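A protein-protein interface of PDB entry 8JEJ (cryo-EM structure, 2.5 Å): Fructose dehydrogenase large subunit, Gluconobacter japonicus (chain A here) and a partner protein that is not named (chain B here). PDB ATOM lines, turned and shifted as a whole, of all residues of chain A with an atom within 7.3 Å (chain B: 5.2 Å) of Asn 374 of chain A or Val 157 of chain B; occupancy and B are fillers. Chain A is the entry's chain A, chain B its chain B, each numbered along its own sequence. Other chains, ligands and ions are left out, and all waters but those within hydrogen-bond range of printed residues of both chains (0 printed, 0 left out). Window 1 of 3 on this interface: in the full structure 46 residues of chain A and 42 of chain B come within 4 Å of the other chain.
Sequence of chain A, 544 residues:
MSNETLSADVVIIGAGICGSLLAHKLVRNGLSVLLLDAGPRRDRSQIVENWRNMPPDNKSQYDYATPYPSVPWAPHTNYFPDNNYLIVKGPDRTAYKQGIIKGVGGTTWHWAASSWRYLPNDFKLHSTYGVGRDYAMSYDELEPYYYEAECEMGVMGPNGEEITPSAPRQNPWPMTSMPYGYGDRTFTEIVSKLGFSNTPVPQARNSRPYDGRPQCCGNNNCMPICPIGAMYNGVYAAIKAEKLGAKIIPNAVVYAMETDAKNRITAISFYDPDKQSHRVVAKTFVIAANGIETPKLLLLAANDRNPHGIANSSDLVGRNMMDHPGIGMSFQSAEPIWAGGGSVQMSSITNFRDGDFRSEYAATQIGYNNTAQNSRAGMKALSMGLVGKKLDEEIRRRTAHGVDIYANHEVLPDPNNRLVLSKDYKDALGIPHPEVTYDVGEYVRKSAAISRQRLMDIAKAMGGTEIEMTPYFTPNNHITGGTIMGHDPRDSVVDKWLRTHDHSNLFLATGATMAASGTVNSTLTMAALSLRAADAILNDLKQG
The side-chain amide nitrogen (ND2) of Asn 374 of chain A lies within hydrogen-bond range of the backbone carbonyl oxygen (O) of Val 158 of chain B, at 2.8 Å. OG of Ser 375 of chain A sits at hydrogen-bond distance from OH of Tyr 150 of chain B (3.3 Å). The side-chain carboxylate (OD1) of Asp 155 of chain B is in salt-bridge range of the guanidinium group (NH1) of Arg 396 of chain A.
The side-chain amide oxygen of Asn 220 of chain A lies within hydrogen-bond range of the backbone NH of Ala 372 of chain A (2.6 Å). The backbone carbonyl oxygen of Ala 400 of chain A is in hydrogen-bond range of the backbone NH of Trp 338 of chain A, at 3.0 Å. A ring nitrogen (NE2) of His 164 of chain B lies within hydrogen-bond range of the backbone carbonyl oxygen (O) of Val 157 of chain B (3.1 Å).
Among the printed residues, merely in contact across the chains: Lys 59 of chain A with Tyr 150 of chain B, Asn 220 of chain A with Val 158 of chain B, Trp 338 of chain A with Val 156 of chain B, Trp 338 of chain A with Val 157 of chain B, Ala 339 of chain A with Val 157 of chain B, Gly 340 of chain A with Val 158 of chain B, Ala 372 of chain A with Val 157 of chain B, Ala 372 of chain A with Val 158 of chain B, Asn 374 of chain A with Tyr 150 of chain B, Asn 374 of chain A with Val 157 of chain B, Asn 374 of chain A with Pro 160 of chain B, Gly 378 of chain A with Met 149 of chain B, Met 379 of chain A with Met 149 of chain B, Ile 395 of chain A with Met 149 of chain B, Arg 396 of chain A with Ser 153 of chain B, Thr 399 of chain A with Ser 153 of chain B and Thr 399 of chain A with Val 157 of chain B.
Of the printed residues of chain B, Asn 374 of chain A touches Tyr 150, Val 157, Val 158 and Pro 160. Val 157 of chain B touches five residues of chain A. Printed residues of chain B within 4 Å of Gly 340 of chain A: Val 158 (3.3 Å). Of the printed residues of chain B, Gly 378 of chain A touches Met 149. Printed residues of chain B within 4 Å of Met 379 of chain A: Met 149 (3.95 Å). Ile 159 of chain B touches none of the printed residues of chain A. The nearest residue of chain B that does not touch Asn 374 of chain A is Ser 153 of chain B (4.03 Å). The nearest printed residue of chain B that does not touch Thr 399 of chain A is Met 149 of chain B (6.5 Å).
Hydrophobic or aromatic side chains of chain A within 4 Å of the printed part of chain B: Trp 338, Ala 372, Met 379 and Ile 395. Hydrophobic or aromatic side chains of chain B within 4 Å of the printed part of chain A: Met 149, Tyr 150, Val 156, Val 157, Val 158 and Pro 160. Along chain B the printed residues that touch a printed residue of chain A span positions 149 to 160.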
ATOM      1  N   LYS A  59      18.852  16.216   6.744  1.00  0.00           N
ATOM      2  CA  LYS A  59      19.249  17.160   7.783  1.00  0.00           C
ATOM      3  C   LYS A  59      18.608  18.526   7.584  1.00  0.00           C
ATOM      4  O   LYS A  59      18.195  19.166   8.557  1.00  0.00           O
ATOM      5  CB  LYS A  59      20.771  17.316   7.810  1.00  0.00           C
ATOM      6  CG  LYS A  59      21.537  16.093   8.262  1.00  0.00           C
ATOM      7  CD  LYS A  59      23.033  16.312   8.124  1.00  0.00           C
ATOM      8  CE  LYS A  59      23.821  15.159   8.713  1.00  0.00           C
ATOM      9  NZ  LYS A  59      24.655  14.481   7.687  1.00  0.00           N
ATOM     10  N   SER A  60      18.541  18.986   6.333  1.00  0.00           N
ATOM     11  CA  SER A  60      17.919  20.270   6.029  1.00  0.00           C
ATOM     12  C   SER A  60      16.452  20.272   6.428  1.00  0.00           C
ATOM     13  O   SER A  60      15.980  21.184   7.116  1.00  0.00           O
ATOM     14  CB  SER A  60      18.079  20.576   4.540  1.00  0.00           C
ATOM     15  OG  SER A  60      16.871  21.041   3.970  1.00  0.00           O
ATOM     16  N   ASN A 220      24.430  22.276  18.634  1.00  0.00           N
ATOM     17  CA  ASN A 220      23.307  22.668  17.785  1.00  0.00           C
ATOM     18  C   ASN A 220      22.630  21.465  17.134  1.00  0.00           C
ATOM     19  O   ASN A 220      22.055  21.572  16.049  1.00  0.00           O
ATOM     20  CB  ASN A 220      23.755  23.670  16.717  1.00  0.00           C
ATOM     21  CG  ASN A 220      22.635  24.571  16.251  1.00  0.00           C
ATOM     22  OD1 ASN A 220      22.227  24.520  15.094  1.00  0.00           O
ATOM     23  ND2 ASN A 220      22.135  25.407  17.150  1.00  0.00           N
ATOM     24  N   TRP A 338      22.503  34.379  11.035  1.00  0.00           N
ATOM     25  CA  TRP A 338      23.538  33.446  11.487  1.00  0.00           C
ATOM     26  C   TRP A 338      23.010  32.491  12.561  1.00  0.00           C
ATOM     27  O   TRP A 338      23.477  32.475  13.701  1.00  0.00           O
ATOM     28  CB  TRP A 338      24.770  34.202  11.998  1.00  0.00           C
ATOM     29  CG  TRP A 338      25.578  34.922  10.953  1.00  0.00           C
ATOM     30  CD1 TRP A 338      25.725  36.271  10.824  1.00  0.00           C
ATOM     31  CD2 TRP A 338      26.377  34.332   9.919  1.00  0.00           C
ATOM     32  NE1 TRP A 338      26.553  36.560   9.769  1.00  0.00           N
ATOM     33  CE2 TRP A 338      26.967  35.388   9.195  1.00  0.00           C
ATOM     34  CE3 TRP A 338      26.643  33.018   9.527  1.00  0.00           C
ATOM     35  CZ2 TRP A 338      27.809  35.168   8.106  1.00  0.00           C
ATOM     36  CZ3 TRP A 338      27.479  32.803   8.446  1.00  0.00           C
ATOM     37  CH2 TRP A 338      28.050  33.872   7.748  1.00  0.00           C
ATOM     38  N   ALA A 339      22.021  31.689  12.177  1.00  0.00           N
ATOM     39  CA  ALA A 339      21.487  30.685  13.086  1.00  0.00           C
ATOM     40  C   ALA A 339      22.522  29.598  13.351  1.00  0.00           C
ATOM     41  O   ALA A 339      23.289  29.220  12.462  1.00  0.00           O
ATOM     42  CB  ALA A 339      20.214  30.068  12.512  1.00  0.00           C
ATOM     43  N   GLY A 340      22.546  29.099  14.584  1.00  0.00           N
ATOM     44  CA  GLY A 340      23.442  28.012  14.929  1.00  0.00           C
ATOM     45  C   GLY A 340      24.284  28.229  16.169  1.00  0.00           C
ATOM     46  O   GLY A 340      25.039  27.338  16.566  1.00  0.00           O
ATOM     47  N   GLY A 341      24.172  29.399  16.792  1.00  0.00           N
ATOM     48  CA  GLY A 341      24.931  29.687  17.994  1.00  0.00           C
ATOM     49  C   GLY A 341      24.213  29.274  19.261  1.00  0.00           C
ATOM     50  O   GLY A 341      23.202  29.876  19.632  1.00  0.00           O
ATOM     51  N   THR A 371      18.457  26.280  14.785  1.00  0.00           N
ATOM     52  CA  THR A 371      19.211  25.244  14.096  1.00  0.00           C
ATOM     53  C   THR A 371      20.012  25.852  12.954  1.00  0.00           C
ATOM     54  O   THR A 371      19.531  26.734  12.236  1.00  0.00           O
ATOM     55  CB  THR A 371      18.279  24.156  13.568  1.00  0.00           C
ATOM     56  OG1 THR A 371      17.331  23.806  14.581  1.00  0.00           O
ATOM     57  CG2 THR A 371      19.075  22.921  13.185  1.00  0.00           C
ATOM     58  N   ALA A 372      21.249  25.387  12.804  1.00  0.00           N
ATOM     59  CA  ALA A 372      22.117  25.888  11.748  1.00  0.00           C
ATOM     60  C   ALA A 372      21.496  25.636  10.381  1.00  0.00           C
ATOM     61  O   ALA A 372      20.951  24.563  10.115  1.00  0.00           O
ATOM     62  CB  ALA A 372      23.491  25.224  11.835  1.00  0.00           C
ATOM     63  N   GLN A 373      21.578  26.643   9.513  1.00  0.00           N
ATOM     64  CA  GLN A 373      20.999  26.581   8.178  1.00  0.00           C
ATOM     65  C   GLN A 373      22.042  26.279   7.110  1.00  0.00           C
ATOM     66  O   GLN A 373      21.851  26.631   5.944  1.00  0.00           O
ATOM     67  CB  GLN A 373      20.276  27.889   7.861  1.00  0.00           C
ATOM     68  CG  GLN A 373      19.135  28.206   8.808  1.00  0.00           C
ATOM     69  CD  GLN A 373      17.778  28.100   8.147  1.00  0.00           C
ATOM     70  OE1 GLN A 373      17.649  28.269   6.937  1.00  0.00           O
ATOM     71  NE2 GLN A 373      16.755  27.816   8.941  1.00  0.00           N
ATOM     72  N   ASN A 374      23.150  25.642   7.490  1.00  0.00           N
ATOM     73  CA  ASN A 374      24.224  25.366   6.541  1.00  0.00           C
ATOM     74  C   ASN A 374      23.863  24.225   5.594  1.00  0.00           C
ATOM     75  O   ASN A 374      24.119  24.306   4.389  1.00  0.00           O
ATOM     76  CB  ASN A 374      25.516  25.056   7.297  1.00  0.00           C
ATOM     77  CG  ASN A 374      25.282  24.186   8.515  1.00  0.00           C
ATOM     78  OD1 ASN A 374      24.184  23.675   8.726  1.00  0.00           O
ATOM     79  ND2 ASN A 374      26.316  24.020   9.328  1.00  0.00           N
ATOM     80  N   SER A 375      23.279  23.149   6.125  1.00  0.00           N
ATOM     81  CA  SER A 375      22.860  22.035   5.278  1.00  0.00           C
ATOM     82  C   SER A 375      21.743  22.464   4.334  1.00  0.00           C
ATOM     83  O   SER A 375      21.762  22.147   3.136  1.00  0.00           O
ATOM     84  CB  SER A 375      22.413  20.864   6.154  1.00  0.00           C
ATOM     85  OG  SER A 375      22.202  19.697   5.384  1.00  0.00           O
ATOM     86  N   ARG A 376      20.763  23.200   4.863  1.00  0.00           N
ATOM     87  CA  ARG A 376      19.673  23.710   4.041  1.00  0.00           C
ATOM     88  C   ARG A 376      20.188  24.658   2.968  1.00  0.00           C
ATOM     89  O   ARG A 376      19.774  24.576   1.805  1.00  0.00           O
ATOM     90  CB  ARG A 376      18.645  24.408   4.934  1.00  0.00           C
ATOM     91  CG  ARG A 376      17.532  25.122   4.192  1.00  0.00           C
ATOM     92  CD  ARG A 376      16.226  24.355   4.292  1.00  0.00           C
ATOM     93  NE  ARG A 376      15.884  24.044   5.675  1.00  0.00           N
ATOM     94  CZ  ARG A 376      15.008  24.723   6.401  1.00  0.00           C
ATOM     95  NH1 ARG A 376      14.354  25.759   5.904  1.00  0.00           N
ATOM     96  NH2 ARG A 376      14.785  24.354   7.659  1.00  0.00           N
ATOM     97  N   ALA A 377      21.102  25.558   3.338  1.00  0.00           N
ATOM     98  CA  ALA A 377      21.666  26.489   2.367  1.00  0.00           C
ATOM     99  C   ALA A 377      22.436  25.755   1.282  1.00  0.00           C
ATOM    100  O   ALA A 377      22.312  26.081   0.097  1.00  0.00           O
ATOM    101  CB  ALA A 377      22.577  27.493   3.069  1.00  0.00           C
ATOM    102  N   GLY A 378      23.239  24.762   1.667  1.00  0.00           N
ATOM    103  CA  GLY A 378      23.996  24.016   0.678  1.00  0.00           C
ATOM    104  C   GLY A 378      23.102  23.282  -0.298  1.00  0.00           C
ATOM    105  O   GLY A 378      23.302  23.350  -1.513  1.00  0.00           O
ATOM    106  N   MET A 379      22.088  22.581   0.220  1.00  0.00           N
ATOM    107  CA  MET A 379      21.183  21.853  -0.664  1.00  0.00           C
ATOM    108  C   MET A 379      20.418  22.802  -1.580  1.00  0.00           C
ATOM    109  O   MET A 379      20.280  22.539  -2.782  1.00  0.00           O
ATOM    110  CB  MET A 379      20.215  20.997   0.154  1.00  0.00           C
ATOM    111  CG  MET A 379      20.887  19.952   1.033  1.00  0.00           C
ATOM    112  SD  MET A 379      22.159  18.991   0.193  1.00  0.00           S
ATOM    113  CE  MET A 379      21.179  18.137  -1.026  1.00  0.00           C
ATOM    114  N   LYS A 380      19.924  23.917  -1.036  1.00  0.00           N
ATOM    115  CA  LYS A 380      19.175  24.864  -1.854  1.00  0.00           C
ATOM    116  C   LYS A 380      20.051  25.462  -2.945  1.00  0.00           C
ATOM    117  O   LYS A 380      19.643  25.538  -4.108  1.00  0.00           O
ATOM    118  CB  LYS A 380      18.581  25.963  -0.976  1.00  0.00           C
ATOM    119  CG  LYS A 380      18.066  27.158  -1.755  1.00  0.00           C
ATOM    120  CD  LYS A 380      16.688  26.891  -2.330  1.00  0.00           C
ATOM    121  CE  LYS A 380      16.141  28.120  -3.031  1.00  0.00           C
ATOM    122  NZ  LYS A 380      15.769  27.842  -4.442  1.00  0.00           N
ATOM    123  N   ILE A 395      25.884  29.729  -1.004  1.00  0.00           N
ATOM    124  CA  ILE A 395      25.812  28.907   0.201  1.00  0.00           C
ATOM    125  C   ILE A 395      26.030  29.768   1.439  1.00  0.00           C
ATOM    126  O   ILE A 395      25.272  29.688   2.414  1.00  0.00           O
ATOM    127  CB  ILE A 395      26.828  27.750   0.132  1.00  0.00           C
ATOM    128  CG1 ILE A 395      26.460  26.775  -0.985  1.00  0.00           C
ATOM    129  CG2 ILE A 395      26.883  27.011   1.458  1.00  0.00           C
ATOM    130  CD1 ILE A 395      27.582  25.847  -1.378  1.00  0.00           C
ATOM    131  N   ARG A 396      27.057  30.622   1.405  1.00  0.00           N
ATOM    132  CA  ARG A 396      27.365  31.466   2.557  1.00  0.00           C
ATOM    133  C   ARG A 396      26.232  32.444   2.852  1.00  0.00           C
ATOM    134  O   ARG A 396      25.821  32.612   4.008  1.00  0.00           O
ATOM    135  CB  ARG A 396      28.675  32.215   2.314  1.00  0.00           C
ATOM    136  CG  ARG A 396      29.103  33.112   3.460  1.00  0.00           C
ATOM    137  CD  ARG A 396      30.562  33.503   3.327  1.00  0.00           C
ATOM    138  NE  ARG A 396      30.965  34.464   4.345  1.00  0.00           N
ATOM    139  CZ  ARG A 396      31.455  34.136   5.532  1.00  0.00           C
ATOM    140  NH1 ARG A 396      31.610  32.873   5.892  1.00  0.00           N
ATOM    141  NH2 ARG A 396      31.798  35.101   6.381  1.00  0.00           N
ATOM    142  N   ARG A 398      23.051  32.190   2.044  1.00  0.00           N
ATOM    143  CA  ARG A 398      21.830  31.520   2.469  1.00  0.00           C
ATOM    144  C   ARG A 398      21.951  30.949   3.874  1.00  0.00           C
ATOM    145  O   ARG A 398      20.951  30.887   4.597  1.00  0.00           O
ATOM    146  CB  ARG A 398      21.462  30.424   1.471  1.00  0.00           C
ATOM    147  CG  ARG A 398      21.024  30.953   0.122  1.00  0.00           C
ATOM    148  CD  ARG A 398      20.108  29.978  -0.584  1.00  0.00           C
ATOM    149  NE  ARG A 398      19.400  30.613  -1.688  1.00  0.00           N
ATOM    150  CZ  ARG A 398      18.116  30.938  -1.667  1.00  0.00           C
ATOM    151  NH1 ARG A 398      17.360  30.696  -0.609  1.00  0.00           N
ATOM    152  NH2 ARG A 398      17.576  31.521  -2.732  1.00  0.00           N
ATOM    153  N   THR A 399      23.147  30.517   4.288  1.00  0.00           N
ATOM    154  CA  THR A 399      23.284  30.083   5.675  1.00  0.00           C
ATOM    155  C   THR A 399      23.332  31.267   6.631  1.00  0.00           C
ATOM    156  O   THR A 399      22.948  31.130   7.797  1.00  0.00           O
ATOM    157  CB  THR A 399      24.523  29.203   5.864  1.00  0.00           C
ATOM    158  OG1 THR A 399      24.678  28.889   7.253  1.00  0.00           O
ATOM    159  CG2 THR A 399      25.750  29.922   5.412  1.00  0.00           C
ATOM    160  N   ALA A 400      23.791  32.433   6.164  1.00  0.00           N
ATOM    161  CA  ALA A 400      23.747  33.620   7.010  1.00  0.00           C
ATOM    162  C   ALA A 400      22.344  34.204   7.125  1.00  0.00           C
ATOM    163  O   ALA A 400      22.019  34.818   8.145  1.00  0.00           O
ATOM    164  CB  ALA A 400      24.708  34.681   6.477  1.00  0.00           C
ATOM    165  N   MET B 149      30.120  22.037   0.950  1.00  0.00           N
ATOM    166  CA  MET B 149      29.031  22.968   1.213  1.00  0.00           C
ATOM    167  C   MET B 149      28.978  23.435   2.663  1.00  0.00           C
ATOM    168  O   MET B 149      28.263  24.398   2.958  1.00  0.00           O
ATOM    169  CB  MET B 149      27.690  22.341   0.820  1.00  0.00           C
ATOM    170  CG  MET B 149      27.053  21.491   1.895  1.00  0.00           C
ATOM    171  SD  MET B 149      25.519  20.735   1.336  1.00  0.00           S
ATOM    172  CE  MET B 149      25.187  19.645   2.707  1.00  0.00           C
ATOM    173  N   TYR B 150      29.709  22.787   3.567  1.00  0.00           N
ATOM    174  CA  TYR B 150      29.830  23.265   4.936  1.00  0.00           C
ATOM    175  C   TYR B 150      31.013  24.201   5.134  1.00  0.00           C
ATOM    176  O   TYR B 150      31.112  24.833   6.189  1.00  0.00           O
ATOM    177  CB  TYR B 150      29.955  22.086   5.903  1.00  0.00           C
ATOM    178  CG  TYR B 150      28.713  21.237   5.985  1.00  0.00           C
ATOM    179  CD1 TYR B 150      27.530  21.753   6.493  1.00  0.00           C
ATOM    180  CD2 TYR B 150      28.721  19.921   5.547  1.00  0.00           C
ATOM    181  CE1 TYR B 150      26.392  20.981   6.567  1.00  0.00           C
ATOM    182  CE2 TYR B 150      27.587  19.142   5.617  1.00  0.00           C
ATOM    183  CZ  TYR B 150      26.426  19.676   6.128  1.00  0.00           C
ATOM    184  OH  TYR B 150      25.294  18.902   6.198  1.00  0.00           O
ATOM    185  N   SER B 153      30.812  28.539   5.256  1.00  0.00           N
ATOM    186  CA  SER B 153      30.335  29.160   6.485  1.00  0.00           C
ATOM    187  C   SER B 153      31.038  28.627   7.724  1.00  0.00           C
ATOM    188  O   SER B 153      30.573  28.877   8.842  1.00  0.00           O
ATOM    189  CB  SER B 153      28.827  28.962   6.626  1.00  0.00           C
ATOM    190  OG  SER B 153      28.463  27.627   6.325  1.00  0.00           O
ATOM    191  N   ARG B 154      32.147  27.907   7.557  1.00  0.00           N
ATOM    192  CA  ARG B 154      32.777  27.224   8.682  1.00  0.00           C
ATOM    193  C   ARG B 154      33.319  28.197   9.719  1.00  0.00           C
ATOM    194  O   ARG B 154      33.365  27.866  10.908  1.00  0.00           O
ATOM    195  CB  ARG B 154      33.898  26.320   8.180  1.00  0.00           C
ATOM    196  CG  ARG B 154      33.539  24.858   8.168  1.00  0.00           C
ATOM    197  CD  ARG B 154      34.765  24.004   7.971  1.00  0.00           C
ATOM    198  NE  ARG B 154      35.110  23.277   9.183  1.00  0.00           N
ATOM    199  CZ  ARG B 154      35.720  22.101   9.200  1.00  0.00           C
ATOM    200  NH1 ARG B 154      36.066  21.487   8.081  1.00  0.00           N
ATOM    201  NH2 ARG B 154      35.987  21.526  10.369  1.00  0.00           N
ATOM    202  N   ASP B 155      33.746  29.388   9.297  1.00  0.00           N
ATOM    203  CA  ASP B 155      34.323  30.341  10.237  1.00  0.00           C
ATOM    204  C   ASP B 155      33.291  30.903  11.206  1.00  0.00           C
ATOM    205  O   ASP B 155      33.671  31.449  12.246  1.00  0.00           O
ATOM    206  CB  ASP B 155      35.004  31.480   9.480  1.00  0.00           C
ATOM    207  CG  ASP B 155      34.053  32.233   8.575  1.00  0.00           C
ATOM    208  OD1 ASP B 155      33.116  31.606   8.038  1.00  0.00           O
ATOM    209  OD2 ASP B 155      34.243  33.453   8.396  1.00  0.00           O
ATOM    210  N   VAL B 156      32.000  30.779  10.897  1.00  0.00           N
ATOM    211  CA  VAL B 156      30.928  31.299  11.737  1.00  0.00           C
ATOM    212  C   VAL B 156      30.027  30.184  12.253  1.00  0.00           C
ATOM    213  O   VAL B 156      29.767  30.087  13.456  1.00  0.00           O
ATOM    214  CB  VAL B 156      30.096  32.368  10.993  1.00  0.00           C
ATOM    215  CG1 VAL B 156      29.174  33.084  11.960  1.00  0.00           C
ATOM    216  CG2 VAL B 156      31.004  33.361  10.287  1.00  0.00           C
ATOM    217  N   VAL B 157      29.549  29.325  11.357  1.00  0.00           N
ATOM    218  CA  VAL B 157      28.463  28.395  11.656  1.00  0.00           C
ATOM    219  C   VAL B 157      29.030  27.039  12.047  1.00  0.00           C
ATOM    220  O   VAL B 157      30.012  26.563  11.464  1.00  0.00           O
ATOM    221  CB  VAL B 157      27.503  28.274  10.458  1.00  0.00           C
ATOM    222  CG1 VAL B 157      26.336  27.359  10.790  1.00  0.00           C
ATOM    223  CG2 VAL B 157      26.998  29.642  10.064  1.00  0.00           C
ATOM    224  N   VAL B 158      28.403  26.418  13.045  1.00  0.00           N
ATOM    225  CA  VAL B 158      28.805  25.098  13.507  1.00  0.00           C
ATOM    226  C   VAL B 158      28.383  24.039  12.497  1.00  0.00           C
ATOM    227  O   VAL B 158      27.295  24.107  11.909  1.00  0.00           O
ATOM    228  CB  VAL B 158      28.195  24.827  14.894  1.00  0.00           C
ATOM    229  CG1 VAL B 158      26.680  24.978  14.850  1.00  0.00           C
ATOM    230  CG2 VAL B 158      28.576  23.450  15.404  1.00  0.00           C
ATOM    231  N   ILE B 159      29.262  23.069  12.264  1.00  0.00           N
ATOM    232  CA  ILE B 159      28.873  21.813  11.631  1.00  0.00           C
ATOM    233  C   ILE B 159      28.375  20.933  12.770  1.00  0.00           C
ATOM    234  O   ILE B 159      29.189  20.400  13.536  1.00  0.00           O
ATOM    235  CB  ILE B 159      30.039  21.178  10.858  1.00  0.00           C
ATOM    236  CG1 ILE B 159      30.615  22.185   9.863  1.00  0.00           C
ATOM    237  CG2 ILE B 159      29.584  19.922  10.135  1.00  0.00           C
ATOM    238  CD1 ILE B 159      31.801  21.669   9.102  1.00  0.00           C
ATOM    239  N   PRO B 160      27.055  20.739  12.897  1.00  0.00           N
ATOM    240  CA  PRO B 160      26.447  20.454  14.206  1.00  0.00           C
ATOM    241  C   PRO B 160      27.154  19.471  15.132  1.00  0.00           C
ATOM    242  O   PRO B 160      27.571  19.872  16.222  1.00  0.00           O
ATOM    243  CB  PRO B 160      25.062  19.934  13.810  1.00  0.00           C
ATOM    244  CG  PRO B 160      24.729  20.752  12.605  1.00  0.00           C
ATOM    245  CD  PRO B 160      26.032  20.983  11.865  1.00  0.00           C
ATOM    246  N   HIS B 164      32.506  24.041  17.578  1.00  0.00           N
ATOM    247  CA  HIS B 164      33.345  25.220  17.454  1.00  0.00           C
ATOM    248  C   HIS B 164      34.113  25.424  18.761  1.00  0.00           C
ATOM    249  O   HIS B 164      33.920  24.706  19.746  1.00  0.00           O
ATOM    250  CB  HIS B 164      32.497  26.445  17.123  1.00  0.00           C
ATOM    251  CG  HIS B 164      32.498  26.821  15.675  1.00  0.00           C
ATOM    252  ND1 HIS B 164      33.096  27.970  15.206  1.00  0.00           N
ATOM    253  CD2 HIS B 164      31.968  26.204  14.593  1.00  0.00           C
ATOM    254  CE1 HIS B 164      32.938  28.045  13.898  1.00  0.00           C
ATOM    255  NE2 HIS B 164      32.258  26.984  13.500  1.00  0.00           N
